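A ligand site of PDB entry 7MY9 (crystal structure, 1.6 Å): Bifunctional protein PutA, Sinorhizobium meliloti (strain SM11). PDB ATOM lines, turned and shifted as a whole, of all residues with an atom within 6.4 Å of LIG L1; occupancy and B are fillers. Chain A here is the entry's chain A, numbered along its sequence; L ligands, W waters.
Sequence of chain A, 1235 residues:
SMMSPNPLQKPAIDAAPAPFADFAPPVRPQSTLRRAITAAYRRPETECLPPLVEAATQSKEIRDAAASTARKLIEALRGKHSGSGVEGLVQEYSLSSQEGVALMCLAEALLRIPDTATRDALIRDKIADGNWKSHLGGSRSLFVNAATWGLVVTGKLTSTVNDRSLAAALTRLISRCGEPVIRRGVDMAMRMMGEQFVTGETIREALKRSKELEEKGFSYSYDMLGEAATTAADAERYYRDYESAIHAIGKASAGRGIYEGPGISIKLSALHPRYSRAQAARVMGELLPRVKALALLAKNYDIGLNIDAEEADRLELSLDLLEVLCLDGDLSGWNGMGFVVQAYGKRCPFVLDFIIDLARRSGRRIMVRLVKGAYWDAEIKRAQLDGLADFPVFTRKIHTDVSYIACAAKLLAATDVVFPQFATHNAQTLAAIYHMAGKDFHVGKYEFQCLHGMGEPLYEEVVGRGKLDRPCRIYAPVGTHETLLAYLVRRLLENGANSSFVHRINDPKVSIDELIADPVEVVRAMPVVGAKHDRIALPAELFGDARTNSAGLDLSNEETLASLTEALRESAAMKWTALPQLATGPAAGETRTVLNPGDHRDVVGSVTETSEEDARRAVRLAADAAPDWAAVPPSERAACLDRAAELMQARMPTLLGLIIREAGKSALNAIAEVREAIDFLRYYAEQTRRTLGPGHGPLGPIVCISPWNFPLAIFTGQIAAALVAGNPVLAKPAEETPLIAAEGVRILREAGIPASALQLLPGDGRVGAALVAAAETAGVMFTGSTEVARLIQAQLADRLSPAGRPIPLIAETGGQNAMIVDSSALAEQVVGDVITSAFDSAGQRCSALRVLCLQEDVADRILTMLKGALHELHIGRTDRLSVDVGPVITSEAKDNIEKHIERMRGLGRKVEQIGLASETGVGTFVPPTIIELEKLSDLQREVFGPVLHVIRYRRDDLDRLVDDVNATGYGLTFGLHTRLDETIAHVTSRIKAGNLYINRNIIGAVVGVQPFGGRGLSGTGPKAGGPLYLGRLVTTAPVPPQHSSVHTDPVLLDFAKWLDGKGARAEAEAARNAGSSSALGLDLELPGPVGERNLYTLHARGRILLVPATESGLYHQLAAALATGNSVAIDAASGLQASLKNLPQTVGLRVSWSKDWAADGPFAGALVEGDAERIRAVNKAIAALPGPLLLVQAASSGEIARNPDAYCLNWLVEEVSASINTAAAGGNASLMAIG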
ATOM      1  N   ASP A 223     -27.026  22.300 -26.033  1.00  0.00           N
ATOM      2  CA  ASP A 223     -26.022  21.272 -26.276  1.00  0.00           C
ATOM      3  C   ASP A 223     -25.205  21.670 -27.495  1.00  0.00           C
ATOM      4  O   ASP A 223     -25.700  21.638 -28.622  1.00  0.00           O
ATOM      5  CB  ASP A 223     -26.706  19.926 -26.495  1.00  0.00           C
ATOM      6  CG  ASP A 223     -25.737  18.848 -26.944  1.00  0.00           C
ATOM      7  OD1 ASP A 223     -24.535  18.951 -26.644  1.00  0.00           O
ATOM      8  OD2 ASP A 223     -26.198  17.890 -27.602  1.00  0.00           O
ATOM      9  N   LEU A 225     -23.201  20.548 -30.089  1.00  0.00           N
ATOM     10  CA  LEU A 225     -23.162  19.181 -30.587  1.00  0.00           C
ATOM     11  C   LEU A 225     -21.720  18.688 -30.686  1.00  0.00           C
ATOM     12  O   LEU A 225     -20.849  19.389 -31.208  1.00  0.00           O
ATOM     13  CB  LEU A 225     -23.836  19.100 -31.960  1.00  0.00           C
ATOM     14  CG  LEU A 225     -25.359  19.247 -31.955  1.00  0.00           C
ATOM     15  CD1 LEU A 225     -25.838  19.646 -33.341  1.00  0.00           C
ATOM     16  CD2 LEU A 225     -26.012  17.937 -31.493  1.00  0.00           C
ATOM     17  N   GLU A 227     -19.248  14.864 -29.362  1.00  0.00           N
ATOM     18  CA  GLU A 227     -19.073  13.718 -28.492  1.00  0.00           C
ATOM     19  C   GLU A 227     -17.944  12.894 -29.059  1.00  0.00           C
ATOM     20  O   GLU A 227     -17.517  13.094 -30.199  1.00  0.00           O
ATOM     21  CB  GLU A 227     -20.345  12.882 -28.405  1.00  0.00           C
ATOM     22  CG  GLU A 227     -20.791  12.260 -29.715  1.00  0.00           C
ATOM     23  CD  GLU A 227     -22.203  11.718 -29.631  1.00  0.00           C
ATOM     24  OE1 GLU A 227     -23.140  12.528 -29.478  1.00  0.00           O
ATOM     25  OE2 GLU A 227     -22.367  10.478 -29.705  1.00  0.00           O
ATOM     26  N   SER A 265     -25.689  21.643 -21.437  1.00  0.00           N
ATOM     27  CA  SER A 265     -25.449  20.211 -21.260  1.00  0.00           C
ATOM     28  C   SER A 265     -24.140  19.852 -21.932  1.00  0.00           C
ATOM     29  O   SER A 265     -23.821  20.374 -23.010  1.00  0.00           O
ATOM     30  CB  SER A 265     -26.590  19.344 -21.838  1.00  0.00           C
ATOM     31  OG  SER A 265     -27.798  19.515 -21.097  1.00  0.00           O
ATOM     32  N   LYS A 267     -21.091  16.496 -22.675  1.00  0.00           N
ATOM     33  CA  LYS A 267     -20.801  15.075 -22.685  1.00  0.00           C
ATOM     34  C   LYS A 267     -19.344  14.872 -22.305  1.00  0.00           C
ATOM     35  O   LYS A 267     -18.458  15.495 -22.894  1.00  0.00           O
ATOM     36  CB  LYS A 267     -21.068  14.440 -24.057  1.00  0.00           C
ATOM     37  CG  LYS A 267     -22.549  14.380 -24.412  1.00  0.00           C
ATOM     38  CD  LYS A 267     -22.743  13.806 -25.817  1.00  0.00           C
ATOM     39  CE  LYS A 267     -24.221  13.555 -26.111  1.00  0.00           C
ATOM     40  NZ  LYS A 267     -25.047  14.783 -25.935  1.00  0.00           N
ATOM     41  N   ASP A 308     -24.466  14.878 -19.454  1.00  0.00           N
ATOM     42  CA  ASP A 308     -25.279  13.889 -20.171  1.00  0.00           C
ATOM     43  C   ASP A 308     -24.775  12.471 -19.896  1.00  0.00           C
ATOM     44  O   ASP A 308     -23.594  12.266 -19.608  1.00  0.00           O
ATOM     45  CB  ASP A 308     -25.209  14.154 -21.684  1.00  0.00           C
ATOM     46  CG  ASP A 308     -25.996  15.388 -22.132  1.00  0.00           C
ATOM     47  OD1 ASP A 308     -26.797  15.938 -21.368  1.00  0.00           O
ATOM     48  OD2 ASP A 308     -25.793  15.809 -23.299  1.00  0.00           O
ATOM     49  N   ALA A 309     -25.668  11.482 -19.992  1.00  0.00           N
ATOM     50  CA  ALA A 309     -25.291  10.079 -19.807  1.00  0.00           C
ATOM     51  C   ALA A 309     -25.050   9.404 -21.158  1.00  0.00           C
ATOM     52  O   ALA A 309     -25.783   9.631 -22.123  1.00  0.00           O
ATOM     53  CB  ALA A 309     -26.363   9.298 -19.038  1.00  0.00           C
ATOM     54  N   VAL A 340     -27.516  13.139 -15.603  1.00  0.00           N
ATOM     55  CA  VAL A 340     -28.552  12.312 -16.218  1.00  0.00           C
ATOM     56  C   VAL A 340     -28.448  10.906 -15.676  1.00  0.00           C
ATOM     57  O   VAL A 340     -27.350  10.359 -15.525  1.00  0.00           O
ATOM     58  CB  VAL A 340     -28.407  12.320 -17.752  1.00  0.00           C
ATOM     59  CG1 VAL A 340     -29.443  11.371 -18.407  1.00  0.00           C
ATOM     60  CG2 VAL A 340     -28.552  13.728 -18.306  1.00  0.00           C
ATOM     61  N   ARG A 369     -31.604  14.637 -14.132  1.00  0.00           N
ATOM     62  CA  ARG A 369     -32.430  14.459 -15.317  1.00  0.00           C
ATOM     63  C   ARG A 369     -32.696  12.969 -15.508  1.00  0.00           C
ATOM     64  O   ARG A 369     -31.771  12.210 -15.809  1.00  0.00           O
ATOM     65  CB  ARG A 369     -31.765  15.057 -16.557  1.00  0.00           C
ATOM     66  CG  ARG A 369     -32.698  14.944 -17.764  1.00  0.00           C
ATOM     67  CD  ARG A 369     -31.939  15.060 -19.058  1.00  0.00           C
ATOM     68  NE  ARG A 369     -31.404  16.401 -19.231  1.00  0.00           N
ATOM     69  CZ  ARG A 369     -30.375  16.688 -20.015  1.00  0.00           C
ATOM     70  NH1 ARG A 369     -29.760  15.722 -20.683  1.00  0.00           N
ATOM     71  NH2 ARG A 369     -29.949  17.951 -20.103  1.00  0.00           N
ATOM     72  N   ALA A 374     -30.692   6.484 -24.699  1.00  0.00           N
ATOM     73  CA  ALA A 374     -30.509   6.776 -26.117  1.00  0.00           C
ATOM     74  C   ALA A 374     -29.680   5.740 -26.868  1.00  0.00           C
ATOM     75  O   ALA A 374     -29.572   5.870 -28.095  1.00  0.00           O
ATOM     76  CB  ALA A 374     -29.859   8.160 -26.297  1.00  0.00           C
ATOM     77  N   TYR A 375     -29.107   4.747 -26.200  1.00  0.00           N
ATOM     78  CA  TYR A 375     -28.126   3.861 -26.827  1.00  0.00           C
ATOM     79  C   TYR A 375     -28.577   2.403 -26.847  1.00  0.00           C
ATOM     80  O   TYR A 375     -27.746   1.503 -26.869  1.00  0.00           O
ATOM     81  CB  TYR A 375     -26.762   3.947 -26.138  1.00  0.00           C
ATOM     82  CG  TYR A 375     -26.169   5.336 -26.031  1.00  0.00           C
ATOM     83  CD1 TYR A 375     -26.588   6.213 -25.032  1.00  0.00           C
ATOM     84  CD2 TYR A 375     -25.188   5.764 -26.910  1.00  0.00           C
ATOM     85  CE1 TYR A 375     -26.052   7.479 -24.919  1.00  0.00           C
ATOM     86  CE2 TYR A 375     -24.632   7.028 -26.808  1.00  0.00           C
ATOM     87  CZ  TYR A 375     -25.070   7.887 -25.823  1.00  0.00           C
ATOM     88  OH  TYR A 375     -24.524   9.145 -25.708  1.00  0.00           O
ATOM     89  N   LEU A 451     -37.140  17.432 -25.979  1.00  0.00           N
ATOM     90  CA  LEU A 451     -36.130  17.700 -27.003  1.00  0.00           C
ATOM     91  C   LEU A 451     -36.661  18.726 -27.995  1.00  0.00           C
ATOM     92  O   LEU A 451     -37.845  18.712 -28.349  1.00  0.00           O
ATOM     93  CB  LEU A 451     -35.718  16.416 -27.740  1.00  0.00           C
ATOM     94  CG  LEU A 451     -34.951  15.363 -26.922  1.00  0.00           C
ATOM     95  CD1 LEU A 451     -34.512  14.167 -27.747  1.00  0.00           C
ATOM     96  CD2 LEU A 451     -33.751  15.985 -26.242  1.00  0.00           C
ATOM     97  N   TYR A 475     -34.321  20.825 -24.498  1.00  0.00           N
ATOM     98  CA  TYR A 475     -32.936  20.483 -24.834  1.00  0.00           C
ATOM     99  C   TYR A 475     -32.687  20.911 -26.283  1.00  0.00           C
ATOM    100  O   TYR A 475     -33.335  20.392 -27.201  1.00  0.00           O
ATOM    101  CB  TYR A 475     -32.699  18.978 -24.652  1.00  0.00           C
ATOM    102  CG  TYR A 475     -31.250  18.507 -24.779  1.00  0.00           C
ATOM    103  CD1 TYR A 475     -30.681  18.234 -26.020  1.00  0.00           C
ATOM    104  CD2 TYR A 475     -30.462  18.316 -23.647  1.00  0.00           C
ATOM    105  CE1 TYR A 475     -29.356  17.796 -26.137  1.00  0.00           C
ATOM    106  CE2 TYR A 475     -29.137  17.885 -23.746  1.00  0.00           C
ATOM    107  CZ  TYR A 475     -28.591  17.638 -24.996  1.00  0.00           C
ATOM    108  OH  TYR A 475     -27.284  17.199 -25.081  1.00  0.00           O
ATOM    109  N   ALA A 486     -24.470  12.199 -35.690  1.00  0.00           N
ATOM    110  CA  ALA A 486     -24.711  11.143 -34.709  1.00  0.00           C
ATOM    111  C   ALA A 486     -25.965  11.424 -33.891  1.00  0.00           C
ATOM    112  O   ALA A 486     -26.838  10.551 -33.742  1.00  0.00           O
ATOM    113  CB  ALA A 486     -23.493  10.988 -33.788  1.00  0.00           C
ATOM    114  N   TYR A 487     -26.078  12.635 -33.354  1.00  0.00           N
ATOM    115  CA  TYR A 487     -27.276  13.024 -32.610  1.00  0.00           C
ATOM    116  C   TYR A 487     -28.522  12.889 -33.464  1.00  0.00           C
ATOM    117  O   TYR A 487     -29.570  12.418 -32.994  1.00  0.00           O
ATOM    118  CB  TYR A 487     -27.110  14.459 -32.108  1.00  0.00           C
ATOM    119  CG  TYR A 487     -28.331  15.033 -31.434  1.00  0.00           C
ATOM    120  CD1 TYR A 487     -29.317  15.696 -32.165  1.00  0.00           C
ATOM    121  CD2 TYR A 487     -28.486  14.955 -30.055  1.00  0.00           C
ATOM    122  CE1 TYR A 487     -30.425  16.232 -31.542  1.00  0.00           C
ATOM    123  CE2 TYR A 487     -29.585  15.492 -29.432  1.00  0.00           C
ATOM    124  CZ  TYR A 487     -30.559  16.130 -30.176  1.00  0.00           C
ATOM    125  OH  TYR A 487     -31.646  16.666 -29.531  1.00  0.00           O
ATOM    126  N   ARG A 490     -29.859   9.307 -34.025  1.00  0.00           N
ATOM    127  CA  ARG A 490     -30.483   8.791 -32.806  1.00  0.00           C
ATOM    128  C   ARG A 490     -31.894   9.315 -32.635  1.00  0.00           C
ATOM    129  O   ARG A 490     -32.786   8.581 -32.196  1.00  0.00           O
ATOM    130  CB  ARG A 490     -29.619   9.121 -31.573  1.00  0.00           C
ATOM    131  CG  ARG A 490     -28.379   8.229 -31.442  1.00  0.00           C
ATOM    132  CD  ARG A 490     -27.787   8.239 -30.031  1.00  0.00           C
ATOM    133  NE  ARG A 490     -27.362   9.561 -29.596  1.00  0.00           N
ATOM    134  CZ  ARG A 490     -26.130  10.060 -29.736  1.00  0.00           C
ATOM    135  NH1 ARG A 490     -25.181   9.332 -30.306  1.00  0.00           N
ATOM    136  NH2 ARG A 490     -25.857  11.287 -29.306  1.00  0.00           N
ATOM    137  N   ARG A 491     -32.137  10.590 -32.998  1.00  0.00           N
ATOM    138  CA  ARG A 491     -33.485  11.150 -32.894  1.00  0.00           C
ATOM    139  C   ARG A 491     -34.418  10.516 -33.915  1.00  0.00           C
ATOM    140  O   ARG A 491     -35.569  10.196 -33.609  1.00  0.00           O
ATOM    141  CB  ARG A 491     -33.442  12.666 -33.106  1.00  0.00           C
ATOM    142  CG  ARG A 491     -32.448  13.414 -32.257  1.00  0.00           C
ATOM    143  CD  ARG A 491     -32.939  13.607 -30.827  1.00  0.00           C
ATOM    144  NE  ARG A 491     -32.961  12.372 -30.048  1.00  0.00           N
ATOM    145  CZ  ARG A 491     -31.894  11.828 -29.481  1.00  0.00           C
ATOM    146  NH1 ARG A 491     -30.700  12.406 -29.629  1.00  0.00           N
ATOM    147  NH2 ARG A 491     -32.001  10.706 -28.776  1.00  0.00           N
ATOM    148  N   GLU A 494     -35.283   7.041 -32.855  1.00  0.00           N
ATOM    149  CA  GLU A 494     -36.296   7.217 -31.819  1.00  0.00           C
ATOM    150  C   GLU A 494     -37.647   7.566 -32.415  1.00  0.00           C
ATOM    151  O   GLU A 494     -38.681   7.026 -32.016  1.00  0.00           O
ATOM    152  CB  GLU A 494     -35.829   8.290 -30.830  1.00  0.00           C
ATOM    153  CG  GLU A 494     -36.825   8.727 -29.764  1.00  0.00           C
ATOM    154  CD  GLU A 494     -36.297   9.908 -28.935  1.00  0.00           C
ATOM    155  OE1 GLU A 494     -35.169  10.373 -29.221  1.00  0.00           O
ATOM    156  OE2 GLU A 494     -37.000  10.369 -28.010  1.00  0.00           O
HETATM  157  C1  LIG L   1     -28.399  12.200 -27.439  1.00  0.00           C
HETATM  158  C2  LIG L   1     -29.009  12.260 -26.011  1.00  0.00           C
HETATM  159  C3  LIG L   1     -29.183  14.572 -24.532  1.00  0.00           C
HETATM  160  C4  LIG L   1     -30.272  14.593 -25.564  1.00  0.00           C
HETATM  161  O1  LIG L   1     -27.698  13.168 -27.826  1.00  0.00           O
HETATM  162  O2  LIG L   1     -28.643  11.168 -28.104  1.00  0.00           O
HETATM  163  S1  LIG L   1     -28.058  13.228 -24.796  1.00  0.00           S
HETATM  164  S2  LIG L   1     -30.711  12.919 -25.962  1.00  0.00           S
HETATM  165  P1  LG2 L   2     -40.900   6.399 -25.217  1.00  0.00           P
HETATM  166  O1  LG2 L   2     -41.495   6.024 -26.597  1.00  0.00           O
HETATM  167  O2  LG2 L   2     -41.765   6.363 -24.049  1.00  0.00           O
HETATM  168  O3  LG2 L   2     -39.749   5.559 -24.752  1.00  0.00           O
HETATM  169  C1  LG2 L   2     -38.762   5.166 -25.728  1.00  0.00           C
HETATM  170  C2  LG2 L   2     -37.530   4.528 -25.062  1.00  0.00           C
HETATM  171  O4  LG2 L   2     -37.765   3.229 -24.642  1.00  0.00           O
HETATM  172  C3  LG2 L   2     -36.316   4.429 -25.927  1.00  0.00           C
HETATM  173  O5  LG2 L   2     -35.681   5.648 -26.140  1.00  0.00           O
HETATM  174  C4  LG2 L   2     -35.481   3.489 -25.143  1.00  0.00           C
HETATM  175  O6  LG2 L   2     -34.826   4.113 -24.093  1.00  0.00           O
HETATM  176  C5  LG2 L   2     -36.531   2.582 -24.572  1.00  0.00           C
HETATM  177  N1  LG2 L   2     -36.703   1.324 -25.259  1.00  0.00           N
HETATM  178  C6  LG2 L   2     -37.122   1.147 -26.567  1.00  0.00           C
HETATM  179  N2  LG2 L   2     -37.188  -0.163 -26.828  1.00  0.00           N
HETATM  180  C7  LG2 L   2     -36.820  -0.892 -25.712  1.00  0.00           C
HETATM  181  C8  LG2 L   2     -36.713  -2.238 -25.406  1.00  0.00           C
HETATM  182  N3  LG2 L   2     -37.017  -3.231 -26.406  1.00  0.00           N
HETATM  183  N4  LG2 L   2     -36.315  -2.613 -24.189  1.00  0.00           N
HETATM  184  C9  LG2 L   2     -36.024  -1.708 -23.220  1.00  0.00           C
HETATM  185  N5  LG2 L   2     -36.126  -0.386 -23.474  1.00  0.00           N
HETATM  186  C10 LG2 L   2     -36.509   0.049 -24.682  1.00  0.00           C
HETATM  187  N6  LG2 L   2     -30.789   9.593 -23.128  1.00  0.00           N
HETATM  188  C11 LG2 L   2     -29.451   9.263 -22.763  1.00  0.00           C
HETATM  189  O7  LG2 L   2     -29.013   8.024 -22.876  1.00  0.00           O
HETATM  190  N7  LG2 L   2     -28.584  10.221 -22.259  1.00  0.00           N
HETATM  191  C12 LG2 L   2     -28.997  11.520 -22.137  1.00  0.00           C
HETATM  192  O8  LG2 L   2     -28.113  12.414 -21.610  1.00  0.00           O
HETATM  193  C13 LG2 L   2     -30.383  11.927 -22.510  1.00  0.00           C
HETATM  194  N8  LG2 L   2     -30.857  13.240 -22.360  1.00  0.00           N
HETATM  195  C14 LG2 L   2     -32.179  13.532 -22.690  1.00  0.00           C
HETATM  196  C15 LG2 L   2     -32.673  14.849 -22.552  1.00  0.00           C
HETATM  197  C16 LG2 L   2     -33.994  15.121 -22.875  1.00  0.00           C
HETATM  198  C17 LG2 L   2     -34.536  16.523 -22.726  1.00  0.00           C
HETATM  199  C18 LG2 L   2     -34.843  14.119 -23.329  1.00  0.00           C
HETATM  200  C19 LG2 L   2     -36.270  14.431 -23.687  1.00  0.00           C
HETATM  201  C20 LG2 L   2     -34.371  12.815 -23.483  1.00  0.00           C
HETATM  202  C21 LG2 L   2     -33.040  12.534 -23.157  1.00  0.00           C
HETATM  203  N9  LG2 L   2     -32.575  11.195 -23.318  1.00  0.00           N
HETATM  204  C22 LG2 L   2     -31.250  10.881 -22.991  1.00  0.00           C
HETATM  205  C23 LG2 L   2     -33.496  10.120 -23.744  1.00  0.00           C
HETATM  206  C24 LG2 L   2     -33.460   9.646 -25.180  1.00  0.00           C
HETATM  207  O9  LG2 L   2     -32.740  10.535 -25.953  1.00  0.00           O
HETATM  208  C25 LG2 L   2     -34.921   9.530 -25.664  1.00  0.00           C
HETATM  209  O10 LG2 L   2     -35.446  10.777 -25.873  1.00  0.00           O
HETATM  210  C26 LG2 L   2     -35.881   8.825 -24.700  1.00  0.00           C
HETATM  211  O11 LG2 L   2     -35.312   7.641 -24.280  1.00  0.00           O
HETATM  212  C27 LG2 L   2     -37.270   8.628 -25.304  1.00  0.00           C
HETATM  213  O12 LG2 L   2     -38.152   8.300 -24.249  1.00  0.00           O
HETATM  214  P2  LG2 L   2     -39.699   8.768 -24.098  1.00  0.00           P
HETATM  215  O13 LG2 L   2     -40.273   8.792 -22.635  1.00  0.00           O
HETATM  216  O14 LG2 L   2     -39.709  10.104 -24.914  1.00  0.00           O
HETATM  217  O15 LG2 L   2     -40.445   7.829 -25.187  1.00  0.00           O
HETATM  218  O   HOH W   1     -25.558  11.341 -24.357  1.00  0.00           O
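O2 of LIG L1 is in salt-bridge range of NE of Arg 490, 2.5 Å away.
The guanidinium group (NH1) of Arg 491 is in salt-bridge range of an oxygen (O2) of LIG L1 (2.8 Å).
The side-chain amino group (NZ) of Lys 267 lies within salt-bridge range of an oxygen (O1) of LIG L1 (3.6 Å).
An oxygen (O9) of LG2 L2 is in hydrogen-bond range of the guanidinium group of Arg 491 (2.9 Å).
The backbone NH of Ala 374 is in hydrogen-bond range of an oxygen (O7) of LG2 L2 (2.9 Å).
The guanidinium group (NH1) of Arg 369 is in hydrogen-bond range of a nitrogen (N8) of LG2 L2 (3.2 Å).
The backbone NH of Ala 309 lies within hydrogen-bond range of an oxygen (O8) of LG2 L2 (3.1 Å).
N7 of LG2 L2 sits at hydrogen-bond distance from O of Ala 309, at 2.9 Å.
OE2 of Glu 494 lies within hydrogen-bond range of O10 of LG2 L2, 2.7 Å away.
O9 of LG2 L2 lies close to S2 of LIG L1 (3.1 Å).
The side-chain carboxylate (OE1) of Glu 227 is in salt-bridge range of the guanidinium group (NH2) of Arg 490 (3.0 Å).
NE of Arg 491 is in salt-bridge range of OE1 of Glu 494.
The side-chain hydroxyl (OH) of Tyr 475 lies within hydrogen-bond range of the side-chain amino group (NZ) of Lys 267.
OD2 of Asp 308 is in hydrogen-bond range of OH of Tyr 475, 2.7 Å away.
The side-chain carboxylate of Asp 223 is in hydrogen-bond range of the side-chain hydroxyl of Tyr 475.
The side-chain amino group of Lys 267 lies within salt-bridge range of the side-chain carboxylate of Asp 308, at 2.9 Å.
The side-chain carboxylate (OD2) of Asp 223 lies within salt-bridge range of the side-chain amino group (NZ) of Lys 267 (3.7 Å).
The side-chain carboxylate (OD1) of Asp 308 is in salt-bridge range of the guanidinium group (NH1) of Arg 369, 3.0 Å away.
The side-chain carboxylate of Asp 308 sits close to a sulfur (S1) of LIG L1 (3.7 Å).
Ala 374 touches LIG L1.
CD2 of Leu 451 touches C4 of LIG L1, at 3.8 Å.
Tyr 475 touches LIG L1.
Tyr 487 touches LIG L1 (CD2 to O1, 3.0 Å).
Hydrophobic or aromatic side chains that line LIG L1: Ala 374, Leu 451, Tyr 475 and Tyr 487.
Of the 18 residues printed, 8 come within 4 Å of LIG L1.
Water W1 lies within hydrogen-bond range of the side-chain hydroxyl (OH) of Tyr 375, the backbone carbonyl oxygen (O) of Ala 309 and a sulfur (S1) of LIG L1.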
